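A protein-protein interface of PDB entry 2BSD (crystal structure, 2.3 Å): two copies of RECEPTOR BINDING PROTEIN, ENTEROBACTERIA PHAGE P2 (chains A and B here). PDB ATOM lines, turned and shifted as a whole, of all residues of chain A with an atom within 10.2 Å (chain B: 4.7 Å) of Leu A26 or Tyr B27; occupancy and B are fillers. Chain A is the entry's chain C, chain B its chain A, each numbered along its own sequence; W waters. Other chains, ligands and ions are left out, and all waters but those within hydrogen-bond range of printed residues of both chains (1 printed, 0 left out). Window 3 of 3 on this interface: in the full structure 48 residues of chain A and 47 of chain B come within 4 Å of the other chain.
Hydrophobic or aromatic side chains of chain B that line the printed part of chain A: Tyr B27, Ile B61 and Tyr B66. Of the 24 printed residues of chain A, 5 touch a printed residue of chain B. Along chain A the printed residues that touch a printed residue of chain B span positions 22 to 30.
Water W1 bridges OH of Tyr B27 (2.6 Å) and OH of Tyr A27 (2.6 Å).
Among the printed residues, pairs that only touch across the chains: Asn A22 with Tyr B66 (3.7 Å), Lys A25 with Tyr B66 (3.5 Å), Leu A26 with Tyr B27 (3.6 Å), Leu A26 with Ile B61 (3.8 Å), Leu A26 with Tyr B66 (3.8 Å), Met A29 with Thr B31 (3.98 Å), Met A29 with Ile B61 (3.9 Å), Met A29 with Tyr B66 (3.9 Å), Leu A30 with Tyr B27 (3.7 Å) and Leu A30 with Ile B61 (3.9 Å).
The backbone NH (N) of Tyr B66 lies within hydrogen-bond range of the side-chain hydroxyl (OG1) of Thr B7 (2.9 Å). The backbone NH (N) of Gly A19 sits at hydrogen-bond distance from the side-chain amide oxygen (OD1) of Asn A22. The side-chain amino group (NZ) of Lys A25 is in hydrogen-bond range of the side-chain amide oxygen (OD1) of Asn A114 (2.8 Å).
Leu A26 touches Tyr B27, but with the chains exchanged Tyr A27 does not touch Leu B26 (7.7 Å). Leu A26 touches Ile B61, but with the chains exchanged Ile A61 does not touch Leu B26 (12.4 Å). Leu A30 touches Tyr B27, but with the chains exchanged Tyr A27 does not touch Leu B30 (6.4 Å). Leu A30 touches Ile B61, but with the chains exchanged Ile A61 does not touch Leu B30 (9.3 Å). 12 positions are printed for both chains.
The side-chain hydroxyl of Thr B31 sits at hydrogen-bond distance from the backbone carbonyl oxygen of Leu A30 (2.7 Å).
Printed residues of chain B within 4 Å of Asn A22: Tyr B66. Gly A24 touches none of the printed residues of chain B. Printed residues of chain B within 4 Å of Lys A25: Tyr B66 (3.5 Å). Leu A26 touches just these residues of chain B: Tyr B27 (3.6 Å), Ile B61 (3.8 Å) and Tyr B66 (3.8 Å). Printed residues of chain B within 4 Å of Leu A30: Tyr B27 (3.7 Å), Thr B31 (2.7 Å) and Ile B61 (3.9 Å). Arg A65 touches none of the printed residues of chain B. Asp B23 touches none of the printed residues of chain A. No residue of chain A comes within 4 Å of Leu B26. Of chain A, only Leu A26 and Leu A30 come within 4 Å of Tyr B27. No residue of chain A comes within 4 Å of Leu B30. Of chain A, only Met A29 (3.98 Å) and Leu A30 (2.7 Å) come within 4 Å of Thr B31. No residue of chain A comes within 4 Å of Gly B64. Of the printed residues of chain A, Tyr B66 touches Asn A22 (3.7 Å), Lys A25 (3.5 Å), Leu A26 (3.8 Å) and Met A29 (3.9 Å). The nearest residue of chain A that does not touch Tyr B27 is Tyr A27 (4.4 Å).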
ATOM      1  N   THR A   7      20.740  23.156  19.539  1.00  0.00           N
ATOM      2  CA  THR A   7      21.519  22.897  18.321  1.00  0.00           C
ATOM      3  C   THR A   7      21.507  21.406  18.013  1.00  0.00           C
ATOM      4  O   THR A   7      22.559  20.752  17.982  1.00  0.00           O
ATOM      5  CB  THR A   7      22.980  23.371  18.462  1.00  0.00           C
ATOM      6  OG1 THR A   7      23.048  24.518  19.315  1.00  0.00           O
ATOM      7  CG2 THR A   7      23.523  23.870  17.113  1.00  0.00           C
ATOM      8  N   GLY A  19      21.327  22.108   8.309  1.00  0.00           N
ATOM      9  CA  GLY A  19      21.559  21.009   9.234  1.00  0.00           C
ATOM     10  C   GLY A  19      22.299  21.399  10.510  1.00  0.00           C
ATOM     11  O   GLY A  19      23.043  22.388  10.553  1.00  0.00           O
ATOM     12  N   SER A  20      22.091  20.604  11.555  1.00  0.00           N
ATOM     13  CA  SER A  20      22.674  20.865  12.862  1.00  0.00           C
ATOM     14  C   SER A  20      24.203  20.733  12.870  1.00  0.00           C
ATOM     15  O   SER A  20      24.888  21.478  13.580  1.00  0.00           O
ATOM     16  CB  SER A  20      22.062  19.934  13.907  1.00  0.00           C
ATOM     17  OG  SER A  20      20.649  19.987  13.879  1.00  0.00           O
ATOM     18  N   ASN A  21      24.736  19.790  12.095  1.00  0.00           N
ATOM     19  CA  ASN A  21      26.180  19.564  12.096  1.00  0.00           C
ATOM     20  C   ASN A  21      26.978  20.645  11.354  1.00  0.00           C
ATOM     21  O   ASN A  21      28.133  20.900  11.689  1.00  0.00           O
ATOM     22  CB  ASN A  21      26.531  18.149  11.613  1.00  0.00           C
ATOM     23  CG  ASN A  21      26.100  17.889  10.194  1.00  0.00           C
ATOM     24  OD1 ASN A  21      25.009  18.295   9.769  1.00  0.00           O
ATOM     25  ND2 ASN A  21      26.944  17.191   9.446  1.00  0.00           N
ATOM     26  N   ASN A  22      26.351  21.277  10.363  1.00  0.00           N
ATOM     27  CA  ASN A  22      26.928  22.444   9.696  1.00  0.00           C
ATOM     28  C   ASN A  22      26.978  23.642  10.644  1.00  0.00           C
ATOM     29  O   ASN A  22      27.971  24.372  10.676  1.00  0.00           O
ATOM     30  CB  ASN A  22      26.152  22.813   8.426  1.00  0.00           C
ATOM     31  CG  ASN A  22      25.419  21.631   7.822  1.00  0.00           C
ATOM     32  OD1 ASN A  22      24.189  21.590   7.828  1.00  0.00           O
ATOM     33  ND2 ASN A  22      26.174  20.662   7.282  1.00  0.00           N
ATOM     34  N   ASP A  23      25.902  23.828  11.411  1.00  0.00           N
ATOM     35  CA  ASP A  23      25.859  24.829  12.478  1.00  0.00           C
ATOM     36  C   ASP A  23      26.853  24.502  13.592  1.00  0.00           C
ATOM     37  O   ASP A  23      27.500  25.403  14.140  1.00  0.00           O
ATOM     38  CB  ASP A  23      24.444  24.951  13.062  1.00  0.00           C
ATOM     39  CG  ASP A  23      23.501  25.756  12.170  1.00  0.00           C
ATOM     40  OD1 ASP A  23      23.972  26.538  11.313  1.00  0.00           O
ATOM     41  OD2 ASP A  23      22.261  25.677  12.264  1.00  0.00           O
ATOM     42  N   GLY A  24      26.968  23.212  13.920  1.00  0.00           N
ATOM     43  CA  GLY A  24      27.913  22.749  14.921  1.00  0.00           C
ATOM     44  C   GLY A  24      29.324  23.205  14.591  1.00  0.00           C
ATOM     45  O   GLY A  24      30.004  23.819  15.422  1.00  0.00           O
ATOM     46  N   LYS A  25      29.750  22.934  13.360  1.00  0.00           N
ATOM     47  CA  LYS A  25      31.090  23.309  12.916  1.00  0.00           C
ATOM     48  C   LYS A  25      31.273  24.831  12.807  1.00  0.00           C
ATOM     49  O   LYS A  25      32.304  25.366  13.221  1.00  0.00           O
ATOM     50  CB  LYS A  25      31.441  22.595  11.614  1.00  0.00           C
ATOM     51  CG  LYS A  25      31.506  21.088  11.781  1.00  0.00           C
ATOM     52  CD  LYS A  25      31.921  20.399  10.498  1.00  0.00           C
ATOM     53  CE  LYS A  25      30.722  20.089   9.622  1.00  0.00           C
ATOM     54  NZ  LYS A  25      31.116  19.240   8.468  1.00  0.00           N
ATOM     55  N   LEU A  26      30.261  25.518  12.286  1.00  0.00           N
ATOM     56  CA  LEU A  26      30.240  26.981  12.272  1.00  0.00           C
ATOM     57  C   LEU A  26      30.483  27.581  13.668  1.00  0.00           C
ATOM     58  O   LEU A  26      31.336  28.459  13.827  1.00  0.00           O
ATOM     59  CB  LEU A  26      28.917  27.500  11.676  1.00  0.00           C
ATOM     60  CG  LEU A  26      28.463  28.941  11.995  1.00  0.00           C
ATOM     61  CD1 LEU A  26      29.446  29.995  11.490  1.00  0.00           C
ATOM     62  CD2 LEU A  26      27.079  29.204  11.420  1.00  0.00           C
ATOM     63  N   TYR A  27      29.746  27.102  14.669  1.00  0.00           N
ATOM     64  CA  TYR A  27      29.886  27.603  16.041  1.00  0.00           C
ATOM     65  C   TYR A  27      31.263  27.287  16.627  1.00  0.00           C
ATOM     66  O   TYR A  27      31.871  28.141  17.280  1.00  0.00           O
ATOM     67  CB  TYR A  27      28.758  27.082  16.954  1.00  0.00           C
ATOM     68  CG  TYR A  27      27.364  27.532  16.535  1.00  0.00           C
ATOM     69  CD1 TYR A  27      27.175  28.708  15.794  1.00  0.00           C
ATOM     70  CD2 TYR A  27      26.234  26.782  16.874  1.00  0.00           C
ATOM     71  CE1 TYR A  27      25.909  29.115  15.401  1.00  0.00           C
ATOM     72  CE2 TYR A  27      24.954  27.191  16.482  1.00  0.00           C
ATOM     73  CZ  TYR A  27      24.805  28.355  15.748  1.00  0.00           C
ATOM     74  OH  TYR A  27      23.553  28.776  15.361  1.00  0.00           O
ATOM     75  N   MET A  28      31.751  26.071  16.386  1.00  0.00           N
ATOM     76  CA  MET A  28      33.093  25.684  16.830  1.00  0.00           C
ATOM     77  C   MET A  28      34.160  26.632  16.277  1.00  0.00           C
ATOM     78  O   MET A  28      35.069  27.047  17.001  1.00  0.00           O
ATOM     79  CB  MET A  28      33.415  24.238  16.424  1.00  0.00           C
ATOM     80  CG  MET A  28      32.706  23.182  17.265  1.00  0.00           C
ATOM     81  SD  MET A  28      32.969  21.478  16.707  1.00  0.00           S
ATOM     82  CE  MET A  28      34.520  21.142  17.467  1.00  0.00           C
ATOM     83  N   MET A  29      34.047  26.968  14.993  1.00  0.00           N
ATOM     84  CA  MET A  29      35.031  27.820  14.339  1.00  0.00           C
ATOM     85  C   MET A  29      34.908  29.292  14.773  1.00  0.00           C
ATOM     86  O   MET A  29      35.908  30.000  14.826  1.00  0.00           O
ATOM     87  CB  MET A  29      34.940  27.689  12.814  1.00  0.00           C
ATOM     88  CG  MET A  29      35.334  26.307  12.245  1.00  0.00           C
ATOM     89  SD  MET A  29      34.710  26.053  10.545  1.00  0.00           S
ATOM     90  CE  MET A  29      35.873  27.022   9.628  1.00  0.00           C
ATOM     91  N   LEU A  30      33.695  29.748  15.090  1.00  0.00           N
ATOM     92  CA  LEU A  30      33.505  31.118  15.571  1.00  0.00           C
ATOM     93  C   LEU A  30      34.191  31.360  16.918  1.00  0.00           C
ATOM     94  O   LEU A  30      34.886  32.367  17.100  1.00  0.00           O
ATOM     95  CB  LEU A  30      32.018  31.486  15.652  1.00  0.00           C
ATOM     96  CG  LEU A  30      31.236  31.642  14.341  1.00  0.00           C
ATOM     97  CD1 LEU A  30      29.805  32.097  14.616  1.00  0.00           C
ATOM     98  CD2 LEU A  30      31.923  32.584  13.335  1.00  0.00           C
ATOM     99  N   THR A  31      34.011  30.417  17.842  1.00  0.00           N
ATOM    100  CA  THR A  31      34.547  30.532  19.198  1.00  0.00           C
ATOM    101  C   THR A  31      35.968  29.953  19.368  1.00  0.00           C
ATOM    102  O   THR A  31      36.617  30.196  20.392  1.00  0.00           O
ATOM    103  CB  THR A  31      33.542  29.926  20.229  1.00  0.00           C
ATOM    104  OG1 THR A  31      33.889  30.335  21.559  1.00  0.00           O
ATOM    105  CG2 THR A  31      33.631  28.401  20.283  1.00  0.00           C
ATOM    106  N   GLY A  32      36.448  29.209  18.367  1.00  0.00           N
ATOM    107  CA  GLY A  32      37.754  28.571  18.436  1.00  0.00           C
ATOM    108  C   GLY A  32      37.799  27.430  19.449  1.00  0.00           C
ATOM    109  O   GLY A  32      38.637  27.412  20.352  1.00  0.00           O
ATOM    110  N   MET A  33      36.882  26.481  19.312  1.00  0.00           N
ATOM    111  CA  MET A  33      36.891  25.286  20.152  1.00  0.00           C
ATOM    112  C   MET A  33      37.136  24.030  19.313  1.00  0.00           C
ATOM    113  O   MET A  33      36.734  23.971  18.154  1.00  0.00           O
ATOM    114  CB  MET A  33      35.583  25.160  20.955  1.00  0.00           C
ATOM    115  CG  MET A  33      34.334  24.760  20.152  1.00  0.00           C
ATOM    116  SD  MET A  33      32.754  24.763  21.096  1.00  0.00           S
ATOM    117  CE  MET A  33      33.074  23.576  22.316  1.00  0.00           C
ATOM    118  N   TYR A  35      37.054  19.463  19.853  1.00  0.00           N
ATOM    119  CA  TYR A  35      36.154  18.505  20.493  1.00  0.00           C
ATOM    120  C   TYR A  35      36.535  18.151  21.932  1.00  0.00           C
ATOM    121  O   TYR A  35      35.771  17.487  22.632  1.00  0.00           O
ATOM    122  CB  TYR A  35      36.008  17.245  19.631  1.00  0.00           C
ATOM    123  CG  TYR A  35      35.183  17.482  18.382  1.00  0.00           C
ATOM    124  CD1 TYR A  35      33.791  17.645  18.458  1.00  0.00           C
ATOM    125  CD2 TYR A  35      35.788  17.552  17.126  1.00  0.00           C
ATOM    126  CE1 TYR A  35      33.026  17.866  17.314  1.00  0.00           C
ATOM    127  CE2 TYR A  35      35.036  17.775  15.983  1.00  0.00           C
ATOM    128  CZ  TYR A  35      33.656  17.933  16.090  1.00  0.00           C
ATOM    129  OH  TYR A  35      32.911  18.152  14.962  1.00  0.00           O
ATOM    130  N   ILE A  61      28.081  24.356  25.683  1.00  0.00           N
ATOM    131  CA  ILE A  61      28.348  24.075  24.280  1.00  0.00           C
ATOM    132  C   ILE A  61      29.416  22.988  24.202  1.00  0.00           C
ATOM    133  O   ILE A  61      30.512  23.147  24.730  1.00  0.00           O
ATOM    134  CB  ILE A  61      28.790  25.339  23.507  1.00  0.00           C
ATOM    135  CG1 ILE A  61      27.718  26.435  23.595  1.00  0.00           C
ATOM    136  CG2 ILE A  61      29.073  24.994  22.033  1.00  0.00           C
ATOM    137  CD1 ILE A  61      28.185  27.810  23.096  1.00  0.00           C
ATOM    138  N   GLY A  63      30.993  20.237  21.212  1.00  0.00           N
ATOM    139  CA  GLY A  63      31.017  19.951  19.785  1.00  0.00           C
ATOM    140  C   GLY A  63      30.204  20.949  18.966  1.00  0.00           C
ATOM    141  O   GLY A  63      29.601  20.588  17.949  1.00  0.00           O
ATOM    142  N   GLY A  64      30.175  22.202  19.416  1.00  0.00           N
ATOM    143  CA  GLY A  64      29.413  23.236  18.742  1.00  0.00           C
ATOM    144  C   GLY A  64      27.910  23.098  18.923  1.00  0.00           C
ATOM    145  O   GLY A  64      27.150  23.815  18.278  1.00  0.00           O
ATOM    146  N   ARG A  65      27.485  22.188  19.802  1.00  0.00           N
ATOM    147  CA  ARG A  65      26.063  21.964  20.087  1.00  0.00           C
ATOM    148  C   ARG A  65      25.675  22.592  21.427  1.00  0.00           C
ATOM    149  O   ARG A  65      26.286  22.298  22.450  1.00  0.00           O
ATOM    150  CB  ARG A  65      25.734  20.460  20.129  1.00  0.00           C
ATOM    151  CG  ARG A  65      26.230  19.622  18.962  1.00  0.00           C
ATOM    152  CD  ARG A  65      25.809  20.148  17.609  1.00  0.00           C
ATOM    153  NE  ARG A  65      26.035  19.193  16.522  1.00  0.00           N
ATOM    154  CZ  ARG A  65      25.075  18.507  15.901  1.00  0.00           C
ATOM    155  NH1 ARG A  65      23.804  18.629  16.272  1.00  0.00           N
ATOM    156  NH2 ARG A  65      25.390  17.680  14.908  1.00  0.00           N
ATOM    157  N   ASP A 111      34.595  13.300  16.713  1.00  0.00           N
ATOM    158  CA  ASP A 111      34.098  14.288  15.766  1.00  0.00           C
ATOM    159  C   ASP A 111      32.668  13.934  15.340  1.00  0.00           C
ATOM    160  O   ASP A 111      32.467  13.304  14.290  1.00  0.00           O
ATOM    161  CB  ASP A 111      35.046  14.336  14.552  1.00  0.00           C
ATOM    162  CG  ASP A 111      34.698  15.442  13.550  1.00  0.00           C
ATOM    163  OD1 ASP A 111      33.600  16.037  13.620  1.00  0.00           O
ATOM    164  OD2 ASP A 111      35.475  15.780  12.630  1.00  0.00           O
ATOM    165  N   ASN A 113      30.291  15.875  14.259  1.00  0.00           N
ATOM    166  CA  ASN A 113      29.733  16.675  13.165  1.00  0.00           C
ATOM    167  C   ASN A 113      30.134  16.185  11.778  1.00  0.00           C
ATOM    168  O   ASN A 113      29.581  16.646  10.783  1.00  0.00           O
ATOM    169  CB  ASN A 113      30.061  18.158  13.333  1.00  0.00           C
ATOM    170  CG  ASN A 113      29.455  18.748  14.591  1.00  0.00           C
ATOM    171  OD1 ASN A 113      28.248  18.632  14.823  1.00  0.00           O
ATOM    172  ND2 ASN A 113      30.287  19.386  15.410  1.00  0.00           N
ATOM    173  N   ASN A 114      31.079  15.248  11.727  1.00  0.00           N
ATOM    174  CA  ASN A 114      31.577  14.687  10.468  1.00  0.00           C
ATOM    175  C   ASN A 114      31.427  13.175  10.323  1.00  0.00           C
ATOM    176  O   ASN A 114      31.465  12.645   9.211  1.00  0.00           O
ATOM    177  CB  ASN A 114      33.048  15.061  10.259  1.00  0.00           C
ATOM    178  CG  ASN A 114      33.213  16.479   9.768  1.00  0.00           C
ATOM    179  OD1 ASN A 114      32.574  16.893   8.800  1.00  0.00           O
ATOM    180  ND2 ASN A 114      34.064  17.241  10.442  1.00  0.00           N
ATOM    181  N   THR B   7      25.419  29.621   4.848  1.00  0.00           N
ATOM    182  CA  THR B   7      24.982  30.978   5.175  1.00  0.00           C
ATOM    183  C   THR B   7      24.685  31.734   3.885  1.00  0.00           C
ATOM    184  O   THR B   7      25.303  32.764   3.568  1.00  0.00           O
ATOM    185  CB  THR B   7      26.017  31.720   6.019  1.00  0.00           C
ATOM    186  OG1 THR B   7      26.668  30.799   6.905  1.00  0.00           O
ATOM    187  CG2 THR B   7      25.310  32.715   6.951  1.00  0.00           C
ATOM    188  N   ASP B  23      23.010  37.500   9.206  1.00  0.00           N
ATOM    189  CA  ASP B  23      23.734  36.416   9.880  1.00  0.00           C
ATOM    190  C   ASP B  23      25.247  36.522   9.667  1.00  0.00           C
ATOM    191  O   ASP B  23      26.019  36.342  10.604  1.00  0.00           O
ATOM    192  CB  ASP B  23      23.232  35.047   9.415  1.00  0.00           C
ATOM    193  CG  ASP B  23      21.953  34.627  10.117  1.00  0.00           C
ATOM    194  OD1 ASP B  23      21.744  35.029  11.283  1.00  0.00           O
ATOM    195  OD2 ASP B  23      21.097  33.891   9.579  1.00  0.00           O
ATOM    196  N   GLY B  24      25.658  36.821   8.438  1.00  0.00           N
ATOM    197  CA  GLY B  24      27.059  37.044   8.125  1.00  0.00           C
ATOM    198  C   GLY B  24      27.702  38.113   8.999  1.00  0.00           C
ATOM    199  O   GLY B  24      28.786  37.908   9.536  1.00  0.00           O
ATOM    200  N   LYS B  25      27.033  39.249   9.150  1.00  0.00           N
ATOM    201  CA  LYS B  25      27.562  40.331   9.972  1.00  0.00           C
ATOM    202  C   LYS B  25      27.614  39.943  11.454  1.00  0.00           C
ATOM    203  O   LYS B  25      28.614  40.192  12.125  1.00  0.00           O
ATOM    204  CB  LYS B  25      26.758  41.615   9.755  1.00  0.00           C
ATOM    205  CG  LYS B  25      26.969  42.225   8.376  1.00  0.00           C
ATOM    206  CD  LYS B  25      26.177  43.509   8.191  1.00  0.00           C
ATOM    207  CE  LYS B  25      24.764  43.226   7.710  1.00  0.00           C
ATOM    208  NZ  LYS B  25      24.057  44.477   7.375  1.00  0.00           N
ATOM    209  N   LEU B  26      26.542  39.318  11.940  1.00  0.00           N
ATOM    210  CA  LEU B  26      26.489  38.764  13.294  1.00  0.00           C
ATOM    211  C   LEU B  26      27.684  37.837  13.576  1.00  0.00           C
ATOM    212  O   LEU B  26      28.398  38.029  14.562  1.00  0.00           O
ATOM    213  CB  LEU B  26      25.144  38.045  13.523  1.00  0.00           C
ATOM    214  CG  LEU B  26      24.935  36.976  14.614  1.00  0.00           C
ATOM    215  CD1 LEU B  26      25.184  37.504  16.017  1.00  0.00           C
ATOM    216  CD2 LEU B  26      23.523  36.424  14.515  1.00  0.00           C
ATOM    217  N   TYR B  27      27.904  36.860  12.697  1.00  0.00           N
ATOM    218  CA  TYR B  27      28.998  35.899  12.837  1.00  0.00           C
ATOM    219  C   TYR B  27      30.380  36.561  12.751  1.00  0.00           C
ATOM    220  O   TYR B  27      31.302  36.188  13.489  1.00  0.00           O
ATOM    221  CB  TYR B  27      28.877  34.792  11.784  1.00  0.00           C
ATOM    222  CG  TYR B  27      27.600  33.971  11.853  1.00  0.00           C
ATOM    223  CD1 TYR B  27      26.901  33.813  13.059  1.00  0.00           C
ATOM    224  CD2 TYR B  27      27.093  33.343  10.709  1.00  0.00           C
ATOM    225  CE1 TYR B  27      25.730  33.053  13.124  1.00  0.00           C
ATOM    226  CE2 TYR B  27      25.917  32.580  10.762  1.00  0.00           C
ATOM    227  CZ  TYR B  27      25.250  32.434  11.972  1.00  0.00           C
ATOM    228  OH  TYR B  27      24.101  31.682  12.038  1.00  0.00           O
ATOM    229  N   MET B  28      30.515  37.546  11.859  1.00  0.00           N
ATOM    230  CA  MET B  28      31.753  38.327  11.749  1.00  0.00           C
ATOM    231  C   MET B  28      32.083  39.018  13.066  1.00  0.00           C
ATOM    232  O   MET B  28      33.236  39.082  13.480  1.00  0.00           O
ATOM    233  CB  MET B  28      31.647  39.369  10.630  1.00  0.00           C
ATOM    234  CG  MET B  28      31.789  38.807   9.214  1.00  0.00           C
ATOM    235  SD  MET B  28      31.552  40.044   7.912  1.00  0.00           S
ATOM    236  CE  MET B  28      33.166  40.870   7.980  1.00  0.00           C
ATOM    237  N   MET B  29      31.053  39.521  13.728  1.00  0.00           N
ATOM    238  CA  MET B  29      31.211  40.251  14.980  1.00  0.00           C
ATOM    239  C   MET B  29      31.487  39.316  16.158  1.00  0.00           C
ATOM    240  O   MET B  29      32.272  39.647  17.050  1.00  0.00           O
ATOM    241  CB  MET B  29      29.972  41.106  15.246  1.00  0.00           C
ATOM    242  CG  MET B  29      29.835  42.278  14.282  1.00  0.00           C
ATOM    243  SD  MET B  29      28.222  43.061  14.313  1.00  0.00           S
ATOM    244  CE  MET B  29      28.333  43.964  15.843  1.00  0.00           C
ATOM    245  N   LEU B  30      30.844  38.149  16.156  1.00  0.00           N
ATOM    246  CA  LEU B  30      31.049  37.167  17.226  1.00  0.00           C
ATOM    247  C   LEU B  30      32.499  36.686  17.299  1.00  0.00           C
ATOM    248  O   LEU B  30      33.076  36.585  18.383  1.00  0.00           O
ATOM    249  CB  LEU B  30      30.093  35.979  17.064  1.00  0.00           C
ATOM    250  CG  LEU B  30      28.608  36.250  17.350  1.00  0.00           C
ATOM    251  CD1 LEU B  30      27.793  34.953  17.228  1.00  0.00           C
ATOM    252  CD2 LEU B  30      28.384  36.913  18.720  1.00  0.00           C
ATOM    253  N   THR B  31      33.083  36.407  16.135  1.00  0.00           N
ATOM    254  CA  THR B  31      34.428  35.838  16.064  1.00  0.00           C
ATOM    255  C   THR B  31      35.546  36.871  15.863  1.00  0.00           C
ATOM    256  O   THR B  31      36.723  36.526  15.936  1.00  0.00           O
ATOM    257  CB  THR B  31      34.476  34.737  14.971  1.00  0.00           C
ATOM    258  OG1 THR B  31      35.674  33.958  15.119  1.00  0.00           O
ATOM    259  CG2 THR B  31      34.586  35.341  13.566  1.00  0.00           C
ATOM    260  N   ILE B  61      34.803  30.009   6.622  1.00  0.00           N
ATOM    261  CA  ILE B  61      33.959  31.181   6.828  1.00  0.00           C
ATOM    262  C   ILE B  61      34.655  32.378   6.191  1.00  0.00           C
ATOM    263  O   ILE B  61      35.797  32.703   6.535  1.00  0.00           O
ATOM    264  CB  ILE B  61      33.690  31.439   8.337  1.00  0.00           C
ATOM    265  CG1 ILE B  61      33.024  30.222   8.990  1.00  0.00           C
ATOM    266  CG2 ILE B  61      32.814  32.686   8.524  1.00  0.00           C
ATOM    267  CD1 ILE B  61      33.077  30.234  10.498  1.00  0.00           C
ATOM    268  N   GLY B  64      31.732  36.196   6.965  1.00  0.00           N
ATOM    269  CA  GLY B  64      30.774  35.602   7.880  1.00  0.00           C
ATOM    270  C   GLY B  64      29.896  34.535   7.254  1.00  0.00           C
ATOM    271  O   GLY B  64      28.909  34.134   7.861  1.00  0.00           O
ATOM    272  N   TYR B  66      29.392  30.731   6.018  1.00  0.00           N
ATOM    273  CA  TYR B  66      29.908  29.383   6.163  1.00  0.00           C
ATOM    274  C   TYR B  66      29.652  28.557   4.894  1.00  0.00           C
ATOM    275  O   TYR B  66      28.555  28.576   4.328  1.00  0.00           O
ATOM    276  CB  TYR B  66      29.276  28.719   7.388  1.00  0.00           C
ATOM    277  CG  TYR B  66      29.736  27.306   7.622  1.00  0.00           C
ATOM    278  CD1 TYR B  66      30.885  27.038   8.374  1.00  0.00           C
ATOM    279  CD2 TYR B  66      29.021  26.233   7.098  1.00  0.00           C
ATOM    280  CE1 TYR B  66      31.308  25.736   8.590  1.00  0.00           C
ATOM    281  CE2 TYR B  66      29.438  24.935   7.305  1.00  0.00           C
ATOM    282  CZ  TYR B  66      30.582  24.691   8.049  1.00  0.00           C
ATOM    283  OH  TYR B  66      30.993  23.389   8.240  1.00  0.00           O
HETATM  284  O   HOH W   1      22.831  30.988  14.162  1.00  0.00           O
